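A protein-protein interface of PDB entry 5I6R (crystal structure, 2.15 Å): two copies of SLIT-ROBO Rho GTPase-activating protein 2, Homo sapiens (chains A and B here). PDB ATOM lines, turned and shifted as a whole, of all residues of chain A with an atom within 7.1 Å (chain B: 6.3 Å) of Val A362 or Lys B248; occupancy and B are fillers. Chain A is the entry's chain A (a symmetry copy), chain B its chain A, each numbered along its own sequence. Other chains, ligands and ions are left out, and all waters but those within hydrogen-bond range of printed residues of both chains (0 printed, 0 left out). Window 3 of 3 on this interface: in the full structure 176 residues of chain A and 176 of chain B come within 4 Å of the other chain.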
ATOM      1  N   CYS A 357     -32.281   7.118 -10.759  1.00  0.00           N
ATOM      2  CA  CYS A 357     -31.755   5.764 -10.753  1.00  0.00           C
ATOM      3  C   CYS A 357     -31.817   5.284  -9.313  1.00  0.00           C
ATOM      4  O   CYS A 357     -31.170   5.851  -8.440  1.00  0.00           O
ATOM      5  CB  CYS A 357     -30.339   5.729 -11.330  1.00  0.00           C
ATOM      6  SG  CYS A 357     -29.432   4.185 -11.054  1.00  0.00           S
ATOM      7  N   ALA A 358     -32.636   4.266  -9.060  1.00  0.00           N
ATOM      8  CA  ALA A 358     -32.838   3.758  -7.697  1.00  0.00           C
ATOM      9  C   ALA A 358     -32.359   2.310  -7.533  1.00  0.00           C
ATOM     10  O   ALA A 358     -32.958   1.520  -6.789  1.00  0.00           O
ATOM     11  CB  ALA A 358     -34.294   3.908  -7.285  1.00  0.00           C
ATOM     12  N   GLN A 359     -31.281   1.981  -8.244  1.00  0.00           N
ATOM     13  CA  GLN A 359     -30.603   0.694  -8.135  1.00  0.00           C
ATOM     14  C   GLN A 359     -29.702   0.695  -6.912  1.00  0.00           C
ATOM     15  O   GLN A 359     -29.396   1.752  -6.370  1.00  0.00           O
ATOM     16  CB  GLN A 359     -29.741   0.450  -9.368  1.00  0.00           C
ATOM     17  CG  GLN A 359     -30.483   0.456 -10.689  1.00  0.00           C
ATOM     18  CD  GLN A 359     -29.579   0.143 -11.868  1.00  0.00           C
ATOM     19  OE1 GLN A 359     -30.051  -0.309 -12.911  1.00  0.00           O
ATOM     20  NE2 GLN A 359     -28.275   0.384 -11.714  1.00  0.00           N
ATOM     21  N   GLN A 360     -29.271  -0.486  -6.481  1.00  0.00           N
ATOM     22  CA  GLN A 360     -28.270  -0.600  -5.425  1.00  0.00           C
ATOM     23  C   GLN A 360     -26.915  -0.096  -5.956  1.00  0.00           C
ATOM     24  O   GLN A 360     -26.635  -0.294  -7.143  1.00  0.00           O
ATOM     25  CB  GLN A 360     -28.182  -2.043  -4.915  1.00  0.00           C
ATOM     26  CG  GLN A 360     -29.469  -2.580  -4.288  1.00  0.00           C
ATOM     27  CD  GLN A 360     -29.944  -1.834  -3.032  1.00  0.00           C
ATOM     28  OE1 GLN A 360     -31.092  -2.001  -2.609  1.00  0.00           O
ATOM     29  NE2 GLN A 360     -29.070  -1.019  -2.429  1.00  0.00           N
ATOM     30  N   PRO A 361     -26.090   0.574  -5.134  1.00  0.00           N
ATOM     31  CA  PRO A 361     -26.329   0.821  -3.702  1.00  0.00           C
ATOM     32  C   PRO A 361     -27.191   2.046  -3.369  1.00  0.00           C
ATOM     33  O   PRO A 361     -27.584   2.212  -2.201  1.00  0.00           O
ATOM     34  CB  PRO A 361     -24.915   1.044  -3.161  1.00  0.00           C
ATOM     35  CG  PRO A 361     -24.184   1.660  -4.306  1.00  0.00           C
ATOM     36  CD  PRO A 361     -24.736   1.004  -5.540  1.00  0.00           C
ATOM     37  N   VAL A 362     -27.485   2.879  -4.372  1.00  0.00           N
ATOM     38  CA  VAL A 362     -28.139   4.185  -4.135  1.00  0.00           C
ATOM     39  C   VAL A 362     -29.591   4.105  -3.622  1.00  0.00           C
ATOM     40  O   VAL A 362     -30.096   5.077  -3.047  1.00  0.00           O
ATOM     41  CB  VAL A 362     -27.996   5.189  -5.330  1.00  0.00           C
ATOM     42  CG1 VAL A 362     -26.537   5.443  -5.676  1.00  0.00           C
ATOM     43  CG2 VAL A 362     -28.750   4.734  -6.564  1.00  0.00           C
ATOM     44  N   GLN A 363     -30.233   2.947  -3.812  1.00  0.00           N
ATOM     45  CA  GLN A 363     -31.624   2.737  -3.414  1.00  0.00           C
ATOM     46  C   GLN A 363     -31.850   2.969  -1.932  1.00  0.00           C
ATOM     47  O   GLN A 363     -32.811   3.652  -1.557  1.00  0.00           O
ATOM     48  CB  GLN A 363     -32.101   1.335  -3.769  1.00  0.00           C
ATOM     49  CG  GLN A 363     -33.618   1.174  -3.693  1.00  0.00           C
ATOM     50  CD  GLN A 363     -34.064  -0.256  -3.435  1.00  0.00           C
ATOM     51  OE1 GLN A 363     -33.557  -1.205  -4.038  1.00  0.00           O
ATOM     52  NE2 GLN A 363     -35.028  -0.416  -2.537  1.00  0.00           N
ATOM     53  N   SER A 364     -30.972   2.408  -1.099  1.00  0.00           N
ATOM     54  CA  SER A 364     -31.121   2.501   0.356  1.00  0.00           C
ATOM     55  C   SER A 364     -31.142   3.961   0.797  1.00  0.00           C
ATOM     56  O   SER A 364     -32.065   4.371   1.482  1.00  0.00           O
ATOM     57  CB  SER A 364     -30.039   1.696   1.103  1.00  0.00           C
ATOM     58  OG  SER A 364     -28.785   2.373   1.126  1.00  0.00           O
ATOM     59  N   GLU A 365     -30.142   4.735   0.372  1.00  0.00           N
ATOM     60  CA  GLU A 365     -30.072   6.163   0.693  1.00  0.00           C
ATOM     61  C   GLU A 365     -31.290   6.965   0.158  1.00  0.00           C
ATOM     62  O   GLU A 365     -31.802   7.843   0.862  1.00  0.00           O
ATOM     63  CB  GLU A 365     -28.719   6.783   0.299  1.00  0.00           C
ATOM     64  CG  GLU A 365     -28.189   6.360  -1.063  1.00  0.00           C
ATOM     65  CD  GLU A 365     -26.667   6.312  -1.152  1.00  0.00           C
ATOM     66  OE1 GLU A 365     -26.033   5.534  -0.405  1.00  0.00           O
ATOM     67  OE2 GLU A 365     -26.101   7.040  -1.994  1.00  0.00           O
ATOM     68  N   LEU A 366     -31.782   6.622  -1.036  1.00  0.00           N
ATOM     69  CA  LEU A 366     -33.013   7.239  -1.562  1.00  0.00           C
ATOM     70  C   LEU A 366     -34.256   6.915  -0.736  1.00  0.00           C
ATOM     71  O   LEU A 366     -35.104   7.776  -0.531  1.00  0.00           O
ATOM     72  CB  LEU A 366     -33.228   6.915  -3.042  1.00  0.00           C
ATOM     73  CG  LEU A 366     -32.179   7.476  -4.018  1.00  0.00           C
ATOM     74  CD1 LEU A 366     -32.437   6.941  -5.422  1.00  0.00           C
ATOM     75  CD2 LEU A 366     -32.117   9.006  -4.038  1.00  0.00           C
ATOM     76  N   VAL A 367     -34.337   5.683  -0.243  1.00  0.00           N
ATOM     77  CA  VAL A 367     -35.414   5.257   0.650  1.00  0.00           C
ATOM     78  C   VAL A 367     -35.337   6.030   1.974  1.00  0.00           C
ATOM     79  O   VAL A 367     -36.360   6.520   2.494  1.00  0.00           O
ATOM     80  CB  VAL A 367     -35.367   3.717   0.860  1.00  0.00           C
ATOM     81  CG1 VAL A 367     -36.205   3.272   2.048  1.00  0.00           C
ATOM     82  CG2 VAL A 367     -35.818   2.997  -0.405  1.00  0.00           C
ATOM     83  N   GLN A 368     -34.117   6.134   2.499  1.00  0.00           N
ATOM     84  CA  GLN A 368     -33.818   6.888   3.719  1.00  0.00           C
ATOM     85  C   GLN A 368     -34.287   8.345   3.574  1.00  0.00           C
ATOM     86  O   GLN A 368     -34.992   8.865   4.433  1.00  0.00           O
ATOM     87  CB  GLN A 368     -32.310   6.853   3.994  1.00  0.00           C
ATOM     88  CG  GLN A 368     -31.941   6.428   5.407  1.00  0.00           C
ATOM     89  CD  GLN A 368     -31.676   4.935   5.518  1.00  0.00           C
ATOM     90  OE1 GLN A 368     -32.461   4.105   5.042  1.00  0.00           O
ATOM     91  NE2 GLN A 368     -30.561   4.585   6.150  1.00  0.00           N
ATOM     92  N   ARG A 369     -33.891   8.957   2.462  1.00  0.00           N
ATOM     93  CA  ARG A 369     -34.227  10.316   2.086  1.00  0.00           C
ATOM     94  C   ARG A 369     -35.736  10.550   1.972  1.00  0.00           C
ATOM     95  O   ARG A 369     -36.268  11.515   2.537  1.00  0.00           O
ATOM     96  CB  ARG A 369     -33.542  10.602   0.759  1.00  0.00           C
ATOM     97  CG  ARG A 369     -33.548  12.050   0.362  1.00  0.00           C
ATOM     98  CD  ARG A 369     -32.239  12.385  -0.302  1.00  0.00           C
ATOM     99  NE  ARG A 369     -32.261  13.778  -0.711  1.00  0.00           N
ATOM    100  CZ  ARG A 369     -31.570  14.267  -1.726  1.00  0.00           C
ATOM    101  NH1 ARG A 369     -31.662  15.549  -2.035  1.00  0.00           N
ATOM    102  NH2 ARG A 369     -30.798  13.463  -2.438  1.00  0.00           N
ATOM    103  N   LEU A 478     -39.846   5.004  -6.001  1.00  0.00           N
ATOM    104  CA  LEU A 478     -39.603   4.015  -4.950  1.00  0.00           C
ATOM    105  C   LEU A 478     -40.823   3.241  -4.503  1.00  0.00           C
ATOM    106  O   LEU A 478     -40.689   2.099  -4.087  1.00  0.00           O
ATOM    107  CB  LEU A 478     -38.937   4.645  -3.715  1.00  0.00           C
ATOM    108  CG  LEU A 478     -37.551   5.279  -3.837  1.00  0.00           C
ATOM    109  CD1 LEU A 478     -37.258   6.028  -2.548  1.00  0.00           C
ATOM    110  CD2 LEU A 478     -36.444   4.279  -4.157  1.00  0.00           C
ATOM    111  N   GLU B 241     -16.555   3.803  -9.401  1.00  0.00           N
ATOM    112  CA  GLU B 241     -16.643   4.937  -8.488  1.00  0.00           C
ATOM    113  C   GLU B 241     -17.235   6.189  -9.185  1.00  0.00           C
ATOM    114  O   GLU B 241     -18.128   6.866  -8.642  1.00  0.00           O
ATOM    115  CB  GLU B 241     -15.250   5.238  -7.915  1.00  0.00           C
ATOM    116  CG  GLU B 241     -15.206   6.371  -6.897  1.00  0.00           C
ATOM    117  CD  GLU B 241     -13.797   6.864  -6.596  1.00  0.00           C
ATOM    118  OE1 GLU B 241     -12.931   6.885  -7.503  1.00  0.00           O
ATOM    119  OE2 GLU B 241     -13.558   7.254  -5.435  1.00  0.00           O
ATOM    120  N   LYS B 243     -18.892   6.425 -12.150  1.00  0.00           N
ATOM    121  CA  LYS B 243     -20.226   6.217 -12.684  1.00  0.00           C
ATOM    122  C   LYS B 243     -21.233   6.472 -11.564  1.00  0.00           C
ATOM    123  O   LYS B 243     -22.268   7.113 -11.794  1.00  0.00           O
ATOM    124  CB  LYS B 243     -20.389   4.800 -13.231  1.00  0.00           C
ATOM    125  CG  LYS B 243     -21.037   4.714 -14.608  1.00  0.00           C
ATOM    126  CD  LYS B 243     -22.479   5.218 -14.660  1.00  0.00           C
ATOM    127  CE  LYS B 243     -22.950   5.405 -16.099  1.00  0.00           C
ATOM    128  NZ  LYS B 243     -24.169   6.257 -16.184  1.00  0.00           N
ATOM    129  N   LEU B 244     -20.885   5.997 -10.359  1.00  0.00           N
ATOM    130  CA  LEU B 244     -21.697   6.145  -9.157  1.00  0.00           C
ATOM    131  C   LEU B 244     -21.847   7.610  -8.737  1.00  0.00           C
ATOM    132  O   LEU B 244     -22.969   8.060  -8.498  1.00  0.00           O
ATOM    133  CB  LEU B 244     -21.132   5.300  -8.012  1.00  0.00           C
ATOM    134  CG  LEU B 244     -22.045   5.092  -6.799  1.00  0.00           C
ATOM    135  CD1 LEU B 244     -23.085   4.016  -7.087  1.00  0.00           C
ATOM    136  CD2 LEU B 244     -21.236   4.740  -5.559  1.00  0.00           C
ATOM    137  N   LYS B 245     -20.728   8.341  -8.660  1.00  0.00           N
ATOM    138  CA  LYS B 245     -20.738   9.790  -8.418  1.00  0.00           C
ATOM    139  C   LYS B 245     -21.668  10.529  -9.379  1.00  0.00           C
ATOM    140  O   LYS B 245     -22.463  11.364  -8.946  1.00  0.00           O
ATOM    141  CB  LYS B 245     -19.334  10.385  -8.516  1.00  0.00           C
ATOM    142  CG  LYS B 245     -18.396  10.027  -7.373  1.00  0.00           C
ATOM    143  CD  LYS B 245     -17.036  10.700  -7.533  1.00  0.00           C
ATOM    144  CE  LYS B 245     -16.983  12.047  -6.822  1.00  0.00           C
ATOM    145  NZ  LYS B 245     -15.675  12.730  -7.018  1.00  0.00           N
ATOM    146  N   ALA B 246     -21.566  10.198 -10.671  1.00  0.00           N
ATOM    147  CA  ALA B 246     -22.367  10.795 -11.742  1.00  0.00           C
ATOM    148  C   ALA B 246     -23.879  10.534 -11.589  1.00  0.00           C
ATOM    149  O   ALA B 246     -24.687  11.470 -11.685  1.00  0.00           O
ATOM    150  CB  ALA B 246     -21.868  10.314 -13.095  1.00  0.00           C
ATOM    151  N   ILE B 247     -24.245   9.271 -11.345  1.00  0.00           N
ATOM    152  CA  ILE B 247     -25.629   8.878 -11.063  1.00  0.00           C
ATOM    153  C   ILE B 247     -26.210   9.714  -9.913  1.00  0.00           C
ATOM    154  O   ILE B 247     -27.283  10.299 -10.059  1.00  0.00           O
ATOM    155  CB  ILE B 247     -25.730   7.362 -10.750  1.00  0.00           C
ATOM    156  CG1 ILE B 247     -25.594   6.536 -12.041  1.00  0.00           C
ATOM    157  CG2 ILE B 247     -27.036   7.015 -10.032  1.00  0.00           C
ATOM    158  CD1 ILE B 247     -25.059   5.131 -11.825  1.00  0.00           C
ATOM    159  N   LYS B 248     -25.486   9.774  -8.790  1.00  0.00           N
ATOM    160  CA  LYS B 248     -25.926  10.522  -7.605  1.00  0.00           C
ATOM    161  C   LYS B 248     -26.130  12.022  -7.892  1.00  0.00           C
ATOM    162  O   LYS B 248     -27.108  12.612  -7.436  1.00  0.00           O
ATOM    163  CB  LYS B 248     -24.978  10.301  -6.418  1.00  0.00           C
ATOM    164  CG  LYS B 248     -25.025   8.883  -5.854  1.00  0.00           C
ATOM    165  CD  LYS B 248     -24.267   8.717  -4.541  1.00  0.00           C
ATOM    166  CE  LYS B 248     -22.826   8.283  -4.773  1.00  0.00           C
ATOM    167  NZ  LYS B 248     -22.201   7.578  -3.615  1.00  0.00           N
ATOM    168  N   ALA B 249     -25.216  12.611  -8.661  1.00  0.00           N
ATOM    169  CA  ALA B 249     -25.293  14.021  -9.049  1.00  0.00           C
ATOM    170  C   ALA B 249     -26.474  14.277 -10.018  1.00  0.00           C
ATOM    171  O   ALA B 249     -27.161  15.289  -9.896  1.00  0.00           O
ATOM    172  CB  ALA B 249     -23.965  14.493  -9.636  1.00  0.00           C
ATOM    173  N   ARG B 250     -26.703  13.344 -10.948  1.00  0.00           N
ATOM    174  CA  ARG B 250     -27.864  13.377 -11.835  1.00  0.00           C
ATOM    175  C   ARG B 250     -29.163  13.338 -11.024  1.00  0.00           C
ATOM    176  O   ARG B 250     -30.100  14.124 -11.285  1.00  0.00           O
ATOM    177  CB  ARG B 250     -27.820  12.214 -12.835  1.00  0.00           C
ATOM    178  CG  ARG B 250     -28.399  12.548 -14.195  1.00  0.00           C
ATOM    179  CD  ARG B 250     -29.345  11.465 -14.689  1.00  0.00           C
ATOM    180  NE  ARG B 250     -28.708  10.171 -14.970  1.00  0.00           N
ATOM    181  CZ  ARG B 250     -27.426   9.979 -15.283  1.00  0.00           C
ATOM    182  NH1 ARG B 250     -26.577  10.991 -15.374  1.00  0.00           N
ATOM    183  NH2 ARG B 250     -26.996   8.752 -15.506  1.00  0.00           N
ATOM    184  N   ASN B 251     -29.214  12.434 -10.042  1.00  0.00           N
ATOM    185  CA  ASN B 251     -30.364  12.304  -9.145  1.00  0.00           C
ATOM    186  C   ASN B 251     -30.625  13.608  -8.372  1.00  0.00           C
ATOM    187  O   ASN B 251     -31.758  14.072  -8.297  1.00  0.00           O
ATOM    188  CB  ASN B 251     -30.159  11.131  -8.177  1.00  0.00           C
ATOM    189  CG  ASN B 251     -30.394   9.768  -8.823  1.00  0.00           C
ATOM    190  OD1 ASN B 251     -30.777   9.667  -9.981  1.00  0.00           O
ATOM    191  ND2 ASN B 251     -30.168   8.710  -8.059  1.00  0.00           N
ATOM    192  N   GLU B 252     -29.556  14.188  -7.822  1.00  0.00           N
ATOM    193  CA  GLU B 252     -29.608  15.481  -7.167  1.00  0.00           C
ATOM    194  C   GLU B 252     -30.180  16.567  -8.079  1.00  0.00           C
ATOM    195  O   GLU B 252     -31.004  17.381  -7.653  1.00  0.00           O
ATOM    196  CB  GLU B 252     -28.217  15.896  -6.688  1.00  0.00           C
ATOM    197  CG  GLU B 252     -27.793  15.306  -5.359  1.00  0.00           C
ATOM    198  CD  GLU B 252     -28.898  15.348  -4.330  1.00  0.00           C
ATOM    199  OE1 GLU B 252     -29.348  16.440  -3.937  1.00  0.00           O
ATOM    200  OE2 GLU B 252     -29.336  14.265  -3.927  1.00  0.00           O
ATOM    201  N   TYR B 253     -29.722  16.560  -9.326  1.00  0.00           N
ATOM    202  CA  TYR B 253     -30.135  17.513 -10.340  1.00  0.00           C
ATOM    203  C   TYR B 253     -31.635  17.382 -10.652  1.00  0.00           C
ATOM    204  O   TYR B 253     -32.360  18.382 -10.642  1.00  0.00           O
ATOM    205  CB  TYR B 253     -29.232  17.379 -11.585  1.00  0.00           C
ATOM    206  CG  TYR B 253     -29.675  18.113 -12.840  1.00  0.00           C
ATOM    207  CD1 TYR B 253     -30.343  19.356 -12.783  1.00  0.00           C
ATOM    208  CD2 TYR B 253     -29.397  17.581 -14.096  1.00  0.00           C
ATOM    209  CE1 TYR B 253     -30.755  20.010 -13.940  1.00  0.00           C
ATOM    210  CE2 TYR B 253     -29.778  18.239 -15.259  1.00  0.00           C
ATOM    211  CZ  TYR B 253     -30.460  19.449 -15.177  1.00  0.00           C
ATOM    212  OH  TYR B 253     -30.831  20.080 -16.326  1.00  0.00           O
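Among the printed residues, pairs that only touch across the chains: Cys A357 with Ile B247 (3.8 Å), Pro A361 with Leu B244 (3.8 Å), Val A362 with Leu B244 (3.99 Å), Val A362 with Lys B248 (3.8 Å), Glu A365 with Lys B248 (3.6 Å) and Leu A366 with Asn B251 (3.9 Å).
Printed residues of chain B within 4 Å of Val A362: Leu B244 and Lys B248.
Of chain A, only Val A362 and Glu A365 come within 4 Å of Lys B248.
Printed residues of chain B within 4 Å of Arg A369: Glu B252 (2.2 Å).
Of the printed residues of chain B, Cys A357 touches Ile B247 and Asn B251.
Of the printed residues of chain A, Leu B244 touches Pro A361 and Val A362.
The nearest printed residue of chain B that does not touch Val A362 is Asn B251 (4.5 Å).
The nearest printed residue of chain B that does not touch Glu A365 is Leu B244 (6.5 Å).
No position is printed for both chains.
Of the 8 pairs that touch across the chains among the printed residues, none has its exchanged pair printed and touching as well.
O of Cys A357 lies within hydrogen-bond range of ND2 of Asn B251 (3.1 Å).
The side-chain carboxylate (OE1) of Glu B252 is in salt-bridge range of the guanidinium group (NH1) of Arg A369, at 3.1 Å.
Of the 12 printed residues of chain B, 5 touch a printed residue of chain A.
Printed residues of chain B that touch a printed residue of chain A: Leu B244, Ile B247, Lys B248, Asn B251 and Glu B252.
Hydrophobic or aromatic side chains of chain B within 4 Å of the printed part of chain A: Leu B244 and Ile B247.
Along chain B the printed residues that touch a printed residue of chain A span positions 244 to 252.
Among the printed residues, 8 pairs touch across the chains.
Among the printed residues, Asp or Glu carboxylates within 4 Å of a Lys or Arg side-chain nitrogen of the other chain: Arg A369 with Glu B252.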
